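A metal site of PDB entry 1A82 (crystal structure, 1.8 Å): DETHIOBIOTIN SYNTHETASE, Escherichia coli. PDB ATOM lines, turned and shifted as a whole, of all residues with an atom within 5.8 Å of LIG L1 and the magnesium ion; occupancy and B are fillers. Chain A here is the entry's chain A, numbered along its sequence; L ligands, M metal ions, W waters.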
ATOM      1  N   ASP A  10      -2.430  -1.891  14.038  1.00  0.00           N
ATOM      2  CA  ASP A  10      -1.250  -1.870  13.173  1.00  0.00           C
ATOM      3  C   ASP A  10      -0.115  -2.547  13.969  1.00  0.00           C
ATOM      4  O   ASP A  10      -0.335  -3.062  15.064  1.00  0.00           O
ATOM      5  CB  ASP A  10      -0.866  -0.401  12.926  1.00  0.00           C
ATOM      6  CG  ASP A  10       0.154  -0.206  11.790  1.00  0.00           C
ATOM      7  OD1 ASP A  10       0.560  -1.181  11.115  1.00  0.00           O
ATOM      8  OD2 ASP A  10       0.519   0.965  11.576  1.00  0.00           O
ATOM      9  N   THR A  11       1.076  -2.587  13.393  1.00  0.00           N
ATOM     10  CA  THR A  11       2.241  -3.091  14.096  1.00  0.00           C
ATOM     11  C   THR A  11       2.701  -1.850  14.901  1.00  0.00           C
ATOM     12  O   THR A  11       2.355  -0.720  14.544  1.00  0.00           O
ATOM     13  CB  THR A  11       3.355  -3.582  13.107  1.00  0.00           C
ATOM     14  OG1 THR A  11       4.481  -4.068  13.854  1.00  0.00           O
ATOM     15  CG2 THR A  11       3.801  -2.454  12.161  1.00  0.00           C
ATOM     16  N   GLU A  12       3.389  -2.068  16.010  1.00  0.00           N
ATOM     17  CA  GLU A  12       3.892  -0.965  16.843  1.00  0.00           C
ATOM     18  C   GLU A  12       2.820  -0.044  17.448  1.00  0.00           C
ATOM     19  O   GLU A  12       3.007   1.157  17.518  1.00  0.00           O
ATOM     20  CB  GLU A  12       4.904  -0.103  16.071  1.00  0.00           C
ATOM     21  CG  GLU A  12       6.288  -0.056  16.718  1.00  0.00           C
ATOM     22  CD  GLU A  12       7.080  -1.354  16.526  1.00  0.00           C
ATOM     23  OE1 GLU A  12       6.472  -2.457  16.553  1.00  0.00           O
ATOM     24  OE2 GLU A  12       8.312  -1.275  16.327  1.00  0.00           O
ATOM     25  N   VAL A  13       1.695  -0.606  17.890  1.00  0.00           N
ATOM     26  CA  VAL A  13       0.667   0.214  18.523  1.00  0.00           C
ATOM     27  C   VAL A  13       0.533  -0.136  19.992  1.00  0.00           C
ATOM     28  O   VAL A  13      -0.227   0.520  20.726  1.00  0.00           O
ATOM     29  CB  VAL A  13      -0.701   0.072  17.819  1.00  0.00           C
ATOM     30  CG1 VAL A  13      -0.595   0.564  16.386  1.00  0.00           C
ATOM     31  CG2 VAL A  13      -1.201  -1.364  17.861  1.00  0.00           C
ATOM     32  N   GLY A  14       1.234  -1.185  20.420  1.00  0.00           N
ATOM     33  CA  GLY A  14       1.213  -1.597  21.813  1.00  0.00           C
ATOM     34  C   GLY A  14       0.632  -2.968  22.142  1.00  0.00           C
ATOM     35  O   GLY A  14       0.289  -3.202  23.300  1.00  0.00           O
ATOM     36  N   LYS A  15       0.505  -3.861  21.167  1.00  0.00           N
ATOM     37  CA  LYS A  15      -0.012  -5.214  21.452  1.00  0.00           C
ATOM     38  C   LYS A  15       0.757  -5.872  22.605  1.00  0.00           C
ATOM     39  O   LYS A  15       0.154  -6.438  23.503  1.00  0.00           O
ATOM     40  CB  LYS A  15       0.068  -6.134  20.218  1.00  0.00           C
ATOM     41  CG  LYS A  15      -0.861  -5.756  19.046  1.00  0.00           C
ATOM     42  CD  LYS A  15      -0.837  -6.834  17.958  1.00  0.00           C
ATOM     43  CE  LYS A  15       0.532  -7.028  17.400  1.00  0.00           C
ATOM     44  NZ  LYS A  15       0.981  -5.776  16.707  1.00  0.00           N
ATOM     45  N   THR A  16       2.083  -5.771  22.573  1.00  0.00           N
ATOM     46  CA  THR A  16       2.917  -6.399  23.611  1.00  0.00           C
ATOM     47  C   THR A  16       2.738  -5.757  24.983  1.00  0.00           C
ATOM     48  O   THR A  16       2.547  -6.460  25.975  1.00  0.00           O
ATOM     49  CB  THR A  16       4.419  -6.455  23.170  1.00  0.00           C
ATOM     50  OG1 THR A  16       4.518  -7.311  22.019  1.00  0.00           O
ATOM     51  CG2 THR A  16       5.322  -7.014  24.279  1.00  0.00           C
ATOM     52  N   VAL A  17       2.764  -4.435  25.052  1.00  0.00           N
ATOM     53  CA  VAL A  17       2.572  -3.743  26.322  1.00  0.00           C
ATOM     54  C   VAL A  17       1.174  -4.092  26.900  1.00  0.00           C
ATOM     55  O   VAL A  17       1.057  -4.426  28.085  1.00  0.00           O
ATOM     56  CB  VAL A  17       2.763  -2.206  26.167  1.00  0.00           C
ATOM     57  CG1 VAL A  17       2.198  -1.443  27.393  1.00  0.00           C
ATOM     58  CG2 VAL A  17       4.239  -1.883  26.027  1.00  0.00           C
ATOM     59  N   ALA A  18       0.136  -4.005  26.084  1.00  0.00           N
ATOM     60  CA  ALA A  18      -1.206  -4.328  26.544  1.00  0.00           C
ATOM     61  C   ALA A  18      -1.312  -5.791  26.950  1.00  0.00           C
ATOM     62  O   ALA A  18      -1.982  -6.099  27.934  1.00  0.00           O
ATOM     63  CB  ALA A  18      -2.233  -4.007  25.491  1.00  0.00           C
ATOM     64  N   LYS A  37       3.165 -16.422  21.657  1.00  0.00           N
ATOM     65  CA  LYS A  37       3.531 -15.614  20.478  1.00  0.00           C
ATOM     66  C   LYS A  37       3.987 -16.674  19.459  1.00  0.00           C
ATOM     67  O   LYS A  37       5.182 -16.861  19.252  1.00  0.00           O
ATOM     68  CB  LYS A  37       4.697 -14.662  20.852  1.00  0.00           C
ATOM     69  CG  LYS A  37       5.247 -13.780  19.719  1.00  0.00           C
ATOM     70  CD  LYS A  37       4.358 -12.564  19.402  1.00  0.00           C
ATOM     71  CE  LYS A  37       4.988 -11.690  18.299  1.00  0.00           C
ATOM     72  NZ  LYS A  37       4.199 -10.426  18.076  1.00  0.00           N
ATOM     73  N   ASP A  54       9.145  -9.687  22.207  1.00  0.00           N
ATOM     74  CA  ASP A  54       7.723  -9.843  22.544  1.00  0.00           C
ATOM     75  C   ASP A  54       7.553 -11.173  23.282  1.00  0.00           C
ATOM     76  O   ASP A  54       6.902 -11.262  24.314  1.00  0.00           O
ATOM     77  CB  ASP A  54       6.855  -9.924  21.284  1.00  0.00           C
ATOM     78  CG  ASP A  54       6.739  -8.606  20.546  1.00  0.00           C
ATOM     79  OD1 ASP A  54       7.532  -7.683  20.802  1.00  0.00           O
ATOM     80  OD2 ASP A  54       5.813  -8.507  19.700  1.00  0.00           O
ATOM     81  N   GLU A 115      -0.592 -13.398  21.325  1.00  0.00           N
ATOM     82  CA  GLU A 115      -0.317 -12.146  20.603  1.00  0.00           C
ATOM     83  C   GLU A 115      -0.048 -12.471  19.124  1.00  0.00           C
ATOM     84  O   GLU A 115       0.663 -13.429  18.814  1.00  0.00           O
ATOM     85  CB  GLU A 115       0.856 -11.354  21.202  1.00  0.00           C
ATOM     86  CG  GLU A 115       1.059 -10.025  20.480  1.00  0.00           C
ATOM     87  CD  GLU A 115       2.348  -9.297  20.831  1.00  0.00           C
ATOM     88  OE1 GLU A 115       2.926  -9.542  21.917  1.00  0.00           O
ATOM     89  OE2 GLU A 115       2.774  -8.445  20.004  1.00  0.00           O
ATOM     90  N   GLY A 116      -0.697 -11.726  18.236  1.00  0.00           N
ATOM     91  CA  GLY A 116      -0.510 -11.934  16.820  1.00  0.00           C
ATOM     92  C   GLY A 116       0.776 -11.240  16.418  1.00  0.00           C
ATOM     93  O   GLY A 116       1.627 -10.984  17.259  1.00  0.00           O
ATOM     94  N   ALA A 117       0.923 -10.944  15.133  1.00  0.00           N
ATOM     95  CA  ALA A 117       2.109 -10.259  14.638  1.00  0.00           C
ATOM     96  C   ALA A 117       1.566  -9.195  13.706  1.00  0.00           C
ATOM     97  O   ALA A 117       0.681  -9.466  12.888  1.00  0.00           O
ATOM     98  CB  ALA A 117       3.037 -11.228  13.884  1.00  0.00           C
ATOM     99  N   GLY A 118       2.048  -7.965  13.868  1.00  0.00           N
ATOM    100  CA  GLY A 118       1.531  -6.889  13.027  1.00  0.00           C
ATOM    101  C   GLY A 118       0.041  -6.661  13.273  1.00  0.00           C
ATOM    102  O   GLY A 118      -0.428  -6.651  14.423  1.00  0.00           O
ATOM    103  N   GLY A 119      -0.706  -6.501  12.198  1.00  0.00           N
ATOM    104  CA  GLY A 119      -2.131  -6.268  12.301  1.00  0.00           C
ATOM    105  C   GLY A 119      -2.916  -7.524  11.986  1.00  0.00           C
ATOM    106  O   GLY A 119      -2.333  -8.600  11.821  1.00  0.00           O
ATOM    107  N   ASN A 175      -4.338   2.254  24.308  1.00  0.00           N
ATOM    108  CA  ASN A 175      -2.954   2.375  24.725  1.00  0.00           C
ATOM    109  C   ASN A 175      -2.389   3.747  24.366  1.00  0.00           C
ATOM    110  O   ASN A 175      -2.387   4.136  23.201  1.00  0.00           O
ATOM    111  CB  ASN A 175      -2.114   1.272  24.095  1.00  0.00           C
ATOM    112  CG  ASN A 175      -0.681   1.303  24.575  1.00  0.00           C
ATOM    113  OD1 ASN A 175      -0.442   1.452  25.757  1.00  0.00           O
ATOM    114  ND2 ASN A 175       0.269   1.168  23.665  1.00  0.00           N
ATOM    115  N   ASP A 176      -1.935   4.492  25.374  1.00  0.00           N
ATOM    116  CA  ASP A 176      -1.395   5.822  25.141  1.00  0.00           C
ATOM    117  C   ASP A 176       0.045   5.726  24.704  1.00  0.00           C
ATOM    118  O   ASP A 176       0.974   5.697  25.519  1.00  0.00           O
ATOM    119  CB  ASP A 176      -1.530   6.681  26.401  1.00  0.00           C
ATOM    120  CG  ASP A 176      -2.971   6.776  26.884  1.00  0.00           C
ATOM    121  OD1 ASP A 176      -3.892   6.392  26.138  1.00  0.00           O
ATOM    122  OD2 ASP A 176      -3.183   7.233  28.028  1.00  0.00           O
ATOM    123  N   VAL A 177       0.236   5.652  23.401  1.00  0.00           N
ATOM    124  CA  VAL A 177       1.553   5.532  22.818  1.00  0.00           C
ATOM    125  C   VAL A 177       2.381   6.809  22.951  1.00  0.00           C
ATOM    126  O   VAL A 177       3.613   6.756  22.941  1.00  0.00           O
ATOM    127  CB  VAL A 177       1.493   5.051  21.337  1.00  0.00           C
ATOM    128  CG1 VAL A 177       1.057   3.603  21.275  1.00  0.00           C
ATOM    129  CG2 VAL A 177       0.520   5.877  20.542  1.00  0.00           C
ATOM    130  N   ILE A 203      -4.005   2.104  29.101  1.00  0.00           N
ATOM    131  CA  ILE A 203      -2.652   2.084  29.626  1.00  0.00           C
ATOM    132  C   ILE A 203      -2.041   3.474  29.399  1.00  0.00           C
ATOM    133  O   ILE A 203      -2.017   3.982  28.279  1.00  0.00           O
ATOM    134  CB  ILE A 203      -1.839   0.969  28.951  1.00  0.00           C
ATOM    135  CG1 ILE A 203      -2.485  -0.385  29.300  1.00  0.00           C
ATOM    136  CG2 ILE A 203      -0.355   1.005  29.374  1.00  0.00           C
ATOM    137  CD1 ILE A 203      -1.849  -1.532  28.628  1.00  0.00           C
ATOM    138  N   PRO A 204      -1.611   4.124  30.481  1.00  0.00           N
ATOM    139  CA  PRO A 204      -1.009   5.466  30.379  1.00  0.00           C
ATOM    140  C   PRO A 204       0.284   5.468  29.586  1.00  0.00           C
ATOM    141  O   PRO A 204       0.881   4.407  29.343  1.00  0.00           O
ATOM    142  CB  PRO A 204      -0.717   5.839  31.845  1.00  0.00           C
ATOM    143  CG  PRO A 204      -1.600   4.932  32.647  1.00  0.00           C
ATOM    144  CD  PRO A 204      -1.626   3.659  31.882  1.00  0.00           C
ATOM    145  N   TRP A 205       0.728   6.658  29.198  1.00  0.00           N
ATOM    146  CA  TRP A 205       2.001   6.811  28.477  1.00  0.00           C
ATOM    147  C   TRP A 205       3.103   6.559  29.502  1.00  0.00           C
ATOM    148  O   TRP A 205       3.321   7.382  30.404  1.00  0.00           O
ATOM    149  CB  TRP A 205       2.132   8.217  27.870  1.00  0.00           C
ATOM    150  CG  TRP A 205       3.484   8.467  27.287  1.00  0.00           C
ATOM    151  CD1 TRP A 205       4.079   7.807  26.230  1.00  0.00           C
ATOM    152  CD2 TRP A 205       4.451   9.393  27.767  1.00  0.00           C
ATOM    153  NE1 TRP A 205       5.359   8.276  26.031  1.00  0.00           N
ATOM    154  CE2 TRP A 205       5.615   9.256  26.963  1.00  0.00           C
ATOM    155  CE3 TRP A 205       4.451  10.344  28.800  1.00  0.00           C
ATOM    156  CZ2 TRP A 205       6.770  10.016  27.170  1.00  0.00           C
ATOM    157  CZ3 TRP A 205       5.606  11.103  29.007  1.00  0.00           C
ATOM    158  CH2 TRP A 205       6.741  10.937  28.198  1.00  0.00           C
ATOM    159  N   LEU A 206       3.756   5.395  29.408  1.00  0.00           N
ATOM    160  CA  LEU A 206       4.818   4.990  30.319  1.00  0.00           C
ATOM    161  C   LEU A 206       6.128   4.892  29.553  1.00  0.00           C
ATOM    162  O   LEU A 206       6.501   3.849  29.009  1.00  0.00           O
ATOM    163  CB  LEU A 206       4.462   3.649  30.969  1.00  0.00           C
ATOM    164  CG  LEU A 206       3.269   3.779  31.923  1.00  0.00           C
ATOM    165  CD1 LEU A 206       2.476   2.481  31.998  1.00  0.00           C
ATOM    166  CD2 LEU A 206       3.765   4.206  33.288  1.00  0.00           C
ATOM    167  N   ALA A 207       6.815   6.023  29.488  1.00  0.00           N
ATOM    168  CA  ALA A 207       8.068   6.159  28.751  1.00  0.00           C
ATOM    169  C   ALA A 207       9.118   5.060  28.939  1.00  0.00           C
ATOM    170  O   ALA A 207       9.584   4.467  27.960  1.00  0.00           O
ATOM    171  CB  ALA A 207       8.672   7.528  29.023  1.00  0.00           C
ATOM    172  N   PRO A 210       7.798   0.092  29.671  1.00  0.00           N
ATOM    173  CA  PRO A 210       6.391  -0.208  29.976  1.00  0.00           C
ATOM    174  C   PRO A 210       6.018  -1.691  29.979  1.00  0.00           C
ATOM    175  O   PRO A 210       4.984  -2.069  30.503  1.00  0.00           O
ATOM    176  CB  PRO A 210       5.630   0.587  28.913  1.00  0.00           C
ATOM    177  CG  PRO A 210       6.569   0.541  27.740  1.00  0.00           C
ATOM    178  CD  PRO A 210       7.916   0.787  28.379  1.00  0.00           C
ATOM    179  N   GLU A 211       6.874  -2.531  29.393  1.00  0.00           N
ATOM    180  CA  GLU A 211       6.629  -3.980  29.345  1.00  0.00           C
ATOM    181  C   GLU A 211       6.813  -4.548  30.748  1.00  0.00           C
ATOM    182  O   GLU A 211       6.222  -5.582  31.098  1.00  0.00           O
ATOM    183  CB  GLU A 211       7.608  -4.694  28.379  1.00  0.00           C
ATOM    184  CG  GLU A 211       7.448  -4.339  26.901  1.00  0.00           C
ATOM    185  CD  GLU A 211       8.042  -2.981  26.514  1.00  0.00           C
ATOM    186  OE1 GLU A 211       8.826  -2.397  27.294  1.00  0.00           O
ATOM    187  OE2 GLU A 211       7.730  -2.472  25.412  1.00  0.00           O
HETATM  188  P1  LIG L   1       4.617  -5.657  16.911  1.00  0.00           P
HETATM  189  O1  LIG L   1       6.100  -5.689  16.719  1.00  0.00           O
HETATM  190  O2  LIG L   1       3.691  -5.674  15.707  1.00  0.00           O
HETATM  191  O3  LIG L   1       4.151  -7.004  17.693  1.00  0.00           O
HETATM  192  P2  LIG L   1       3.297  -4.034  19.112  1.00  0.00           P
HETATM  193  O4  LIG L   1       3.456  -5.219  19.993  1.00  0.00           O
HETATM  194  O5  LIG L   1       1.958  -3.682  18.576  1.00  0.00           O
HETATM  195  O6  LIG L   1       4.283  -4.277  17.871  1.00  0.00           O
HETATM  196  P3  LIG L   1       4.668  -2.733  21.401  1.00  0.00           P
HETATM  197  O7  LIG L   1       3.840  -3.087  22.598  1.00  0.00           O
HETATM  198  O8  LIG L   1       5.962  -3.397  21.176  1.00  0.00           O
HETATM  199  O9  LIG L   1       3.761  -2.843  20.050  1.00  0.00           O
HETATM  200  O10 LIG L   1       4.826  -1.121  21.438  1.00  0.00           O
HETATM  201  C1  LIG L   1       5.593  -0.462  20.409  1.00  0.00           C
HETATM  202  C2  LIG L   1       6.594   0.517  21.029  1.00  0.00           C
HETATM  203  O11 LIG L   1       5.939   1.600  21.734  1.00  0.00           O
HETATM  204  C3  LIG L   1       7.589  -0.120  21.999  1.00  0.00           C
HETATM  205  O12 LIG L   1       8.907   0.447  21.951  1.00  0.00           O
HETATM  206  C4  LIG L   1       6.939   0.156  23.350  1.00  0.00           C
HETATM  207  O13 LIG L   1       7.909   0.132  24.415  1.00  0.00           O
HETATM  208  C5  LIG L   1       6.299   1.519  23.114  1.00  0.00           C
HETATM  209  N1  LIG L   1       5.045   1.626  23.916  1.00  0.00           N
HETATM  210  C6  LIG L   1       3.989   0.828  23.782  1.00  0.00           C
HETATM  211  N2  LIG L   1       3.060   1.192  24.668  1.00  0.00           N
HETATM  212  C7  LIG L   1       3.524   2.230  25.363  1.00  0.00           C
HETATM  213  C8  LIG L   1       3.014   3.001  26.394  1.00  0.00           C
HETATM  214  N3  LIG L   1       1.811   2.776  26.917  1.00  0.00           N
HETATM  215  N4  LIG L   1       3.778   3.995  26.880  1.00  0.00           N
HETATM  216  C9  LIG L   1       4.997   4.241  26.382  1.00  0.00           C
HETATM  217  N5  LIG L   1       5.502   3.514  25.394  1.00  0.00           N
HETATM  218  C10 LIG L   1       4.789   2.515  24.876  1.00  0.00           C
HETATM  219  C1  LG2 L   2       2.040  -5.905   7.121  1.00  0.00           C
HETATM  220  O1  LG2 L   2       0.818  -5.725   7.271  1.00  0.00           O
HETATM  221  O2  LG2 L   2       2.708  -5.287   6.263  1.00  0.00           O
HETATM  222  C2  LG2 L   2       2.721  -6.931   8.005  1.00  0.00           C
HETATM  223  C3  LG2 L   2       3.659  -6.304   9.033  1.00  0.00           C
HETATM  224  C4  LG2 L   2       4.010  -7.279  10.166  1.00  0.00           C
HETATM  225  C5  LG2 L   2       5.107  -6.710  11.036  1.00  0.00           C
HETATM  226  C6  LG2 L   2       5.220  -7.370  12.419  1.00  0.00           C
HETATM  227  C7  LG2 L   2       6.670  -7.445  12.939  1.00  0.00           C
HETATM  228  C8  LG2 L   2       7.332  -6.060  12.913  1.00  0.00           C
HETATM  229  C9  LG2 L   2       8.668  -6.195  12.262  1.00  0.00           C
HETATM  230  N1  LG2 L   2       6.781  -8.143  14.252  1.00  0.00           N
HETATM  231  N2  LG2 L   2       7.472  -5.434  14.274  1.00  0.00           N
HETATM  232 MG    MG M   1       4.257  -7.013  19.873  1.00  0.00          MG
HETATM  233  O   HOH W   1      10.000   1.978  24.715  1.00  0.00           O
HETATM  234  O   HOH W   2       4.528  -8.386  15.762  1.00  0.00           O
HETATM  235  O   HOH W   3       7.922  -8.342  17.427  1.00  0.00           O
HETATM  236  O   HOH W   4       8.331   3.955  25.137  1.00  0.00           O
HETATM  237  O   HOH W   5       7.729  -3.945  23.067  1.00  0.00           O
HETATM  238  O   HOH W   6      10.786  -0.806  26.000  1.00  0.00           O
HETATM  239  O   HOH W   7       6.191  -5.599  19.819  1.00  0.00           O
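Ile 203 touches LIG L1.
Trp 205 touches LIG L1 (CD1 to C9, 3.7 Å).
Pro 210 touches LIG L1 (CG to O13, 3.6 Å).
Hydrophobic or aromatic side chains that line LIG L1: Val 13, Val 17, Ile 203, Trp 205 and Pro 210.
Within 4 Å of LIG L1: Thr 11, Glu 12, Val 13, Gly 14, Lys 15, Thr 16, Val 17, Lys 37, Asp 54, Glu 115, Gly 118, Asn 175, Asp 176, Ile 203, Pro 204, Trp 205, Leu 206, Pro 210 and Glu 211.
Water W7 lies within hydrogen-bond range of O8 of LIG L1 (2.6 Å) and OD1 of Asp 54 (2.7 Å).
Water W2 lies within hydrogen-bond range of a nitrogen (N1) of LG2 L2 (2.7 Å), an oxygen (O2) of LIG L1 (2.8 Å), the side-chain amino group of Lys 37 (3.1 Å) and the backbone NH of Gly 118 (3.1 Å).
Water W5 lies within hydrogen-bond range of an oxygen (O8) of LIG L1 (2.6 Å) and the side-chain carboxylate (OE2) of Glu 211 (2.8 Å).
Water W4 bridges N5 of LIG L1 (2.9 Å) and O of Ala 207 (3.1 Å).
Water W3 lies within hydrogen-bond range of an oxygen (O1) of LIG L1 (3.3 Å), a nitrogen (N1) of LG2 L2 (3.4 Å) and the side-chain carboxylate (OD1) of Asp 54 (3.5 Å).
Water W6 bridges OE1 of Glu 211 (2.8 Å) and O13 of LIG L1 (3.4 Å).
An oxygen (O1) of LIG L1 sits at hydrogen-bond distance from a nitrogen (N2) of LG2 L2.
The magnesium ion is bound by O4 of LIG L1, OE2 of Glu 115, OD2 of Asp 54, OG1 of Thr 16, O3 of LIG L1 and water W7.
Residues that only touch the magnesium ion: Lys 37 (3.9 Å).
Of the 26 residues printed, 4 come within 4 Å of the magnesium ion.
OE2 of Glu 115 lies close to NZ of Lys 37.
The side-chain amino group (NZ) of Lys 37 lies close to the side-chain carboxylate (OD2) of Asp 54.
ND2 of Asn 175 is in hydrogen-bond range of O of Val 13, at 3.1 Å.
The backbone carbonyl oxygen (O) of Gly 118 is in hydrogen-bond range of the side-chain amino group (NZ) of Lys 15.
The backbone carbonyl oxygen (O) of Asp 10 lies within hydrogen-bond range of the side-chain amino group (NZ) of Lys 15 (3.4 Å).
The backbone NH (N) of Asp 176 is in hydrogen-bond range of the backbone carbonyl oxygen (O) of Ile 203 (3.0 Å).
NZ of Lys 37 lies within hydrogen-bond range of O of Gly 116, at 2.8 Å.
N of Thr 16 is in hydrogen-bond range of O7 of LIG L1.
OG1 of Thr 11 sits at hydrogen-bond distance from O2 of LIG L1.
The side-chain carboxylate (OE2) of Glu 211 sits at hydrogen-bond distance from an oxygen (O13) of LIG L1 (2.8 Å).
A nitrogen (N3) of LIG L1 sits at hydrogen-bond distance from the side-chain amide oxygen of Asn 175 (2.9 Å).
N of Lys 15 lies within hydrogen-bond range of O5 of LIG L1 (3.0 Å).
The side-chain amino group of Lys 15 lies within salt-bridge range of an oxygen (O2) of LIG L1 (2.9 Å).
The backbone NH (N) of Leu 206 is in hydrogen-bond range of a nitrogen (N4) of LIG L1 (2.9 Å).
The backbone NH (N) of Val 17 sits at hydrogen-bond distance from an oxygen (O7) of LIG L1 (3.0 Å).
The backbone NH of Glu 12 sits at hydrogen-bond distance from an oxygen (O6) of LIG L1 (3.0 Å).
The backbone NH (N) of Gly 14 sits at hydrogen-bond distance from an oxygen (O9) of LIG L1, 3.0 Å away.
O of Pro 204 sits at hydrogen-bond distance from N3 of LIG L1.
The backbone NH (N) of Val 13 lies within hydrogen-bond range of an oxygen (O5) of LIG L1, at 3.2 Å.
The backbone carbonyl oxygen (O) of Asp 176 lies within hydrogen-bond range of a nitrogen (N3) of LIG L1 (3.3 Å).
N of Gly 118 sits at hydrogen-bond distance from O2 of LIG L1.
The side-chain amino group (NZ) of Lys 37 lies close to an oxygen (O3) of LIG L1 (3.4 Å).
The side-chain hydroxyl (OG1) of Thr 11 sits at hydrogen-bond distance from a nitrogen (N2) of LG2 L2, 3.3 Å away.
OE1 of Glu 12 is in salt-bridge range of N2 of LG2 L2 (3.9 Å).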
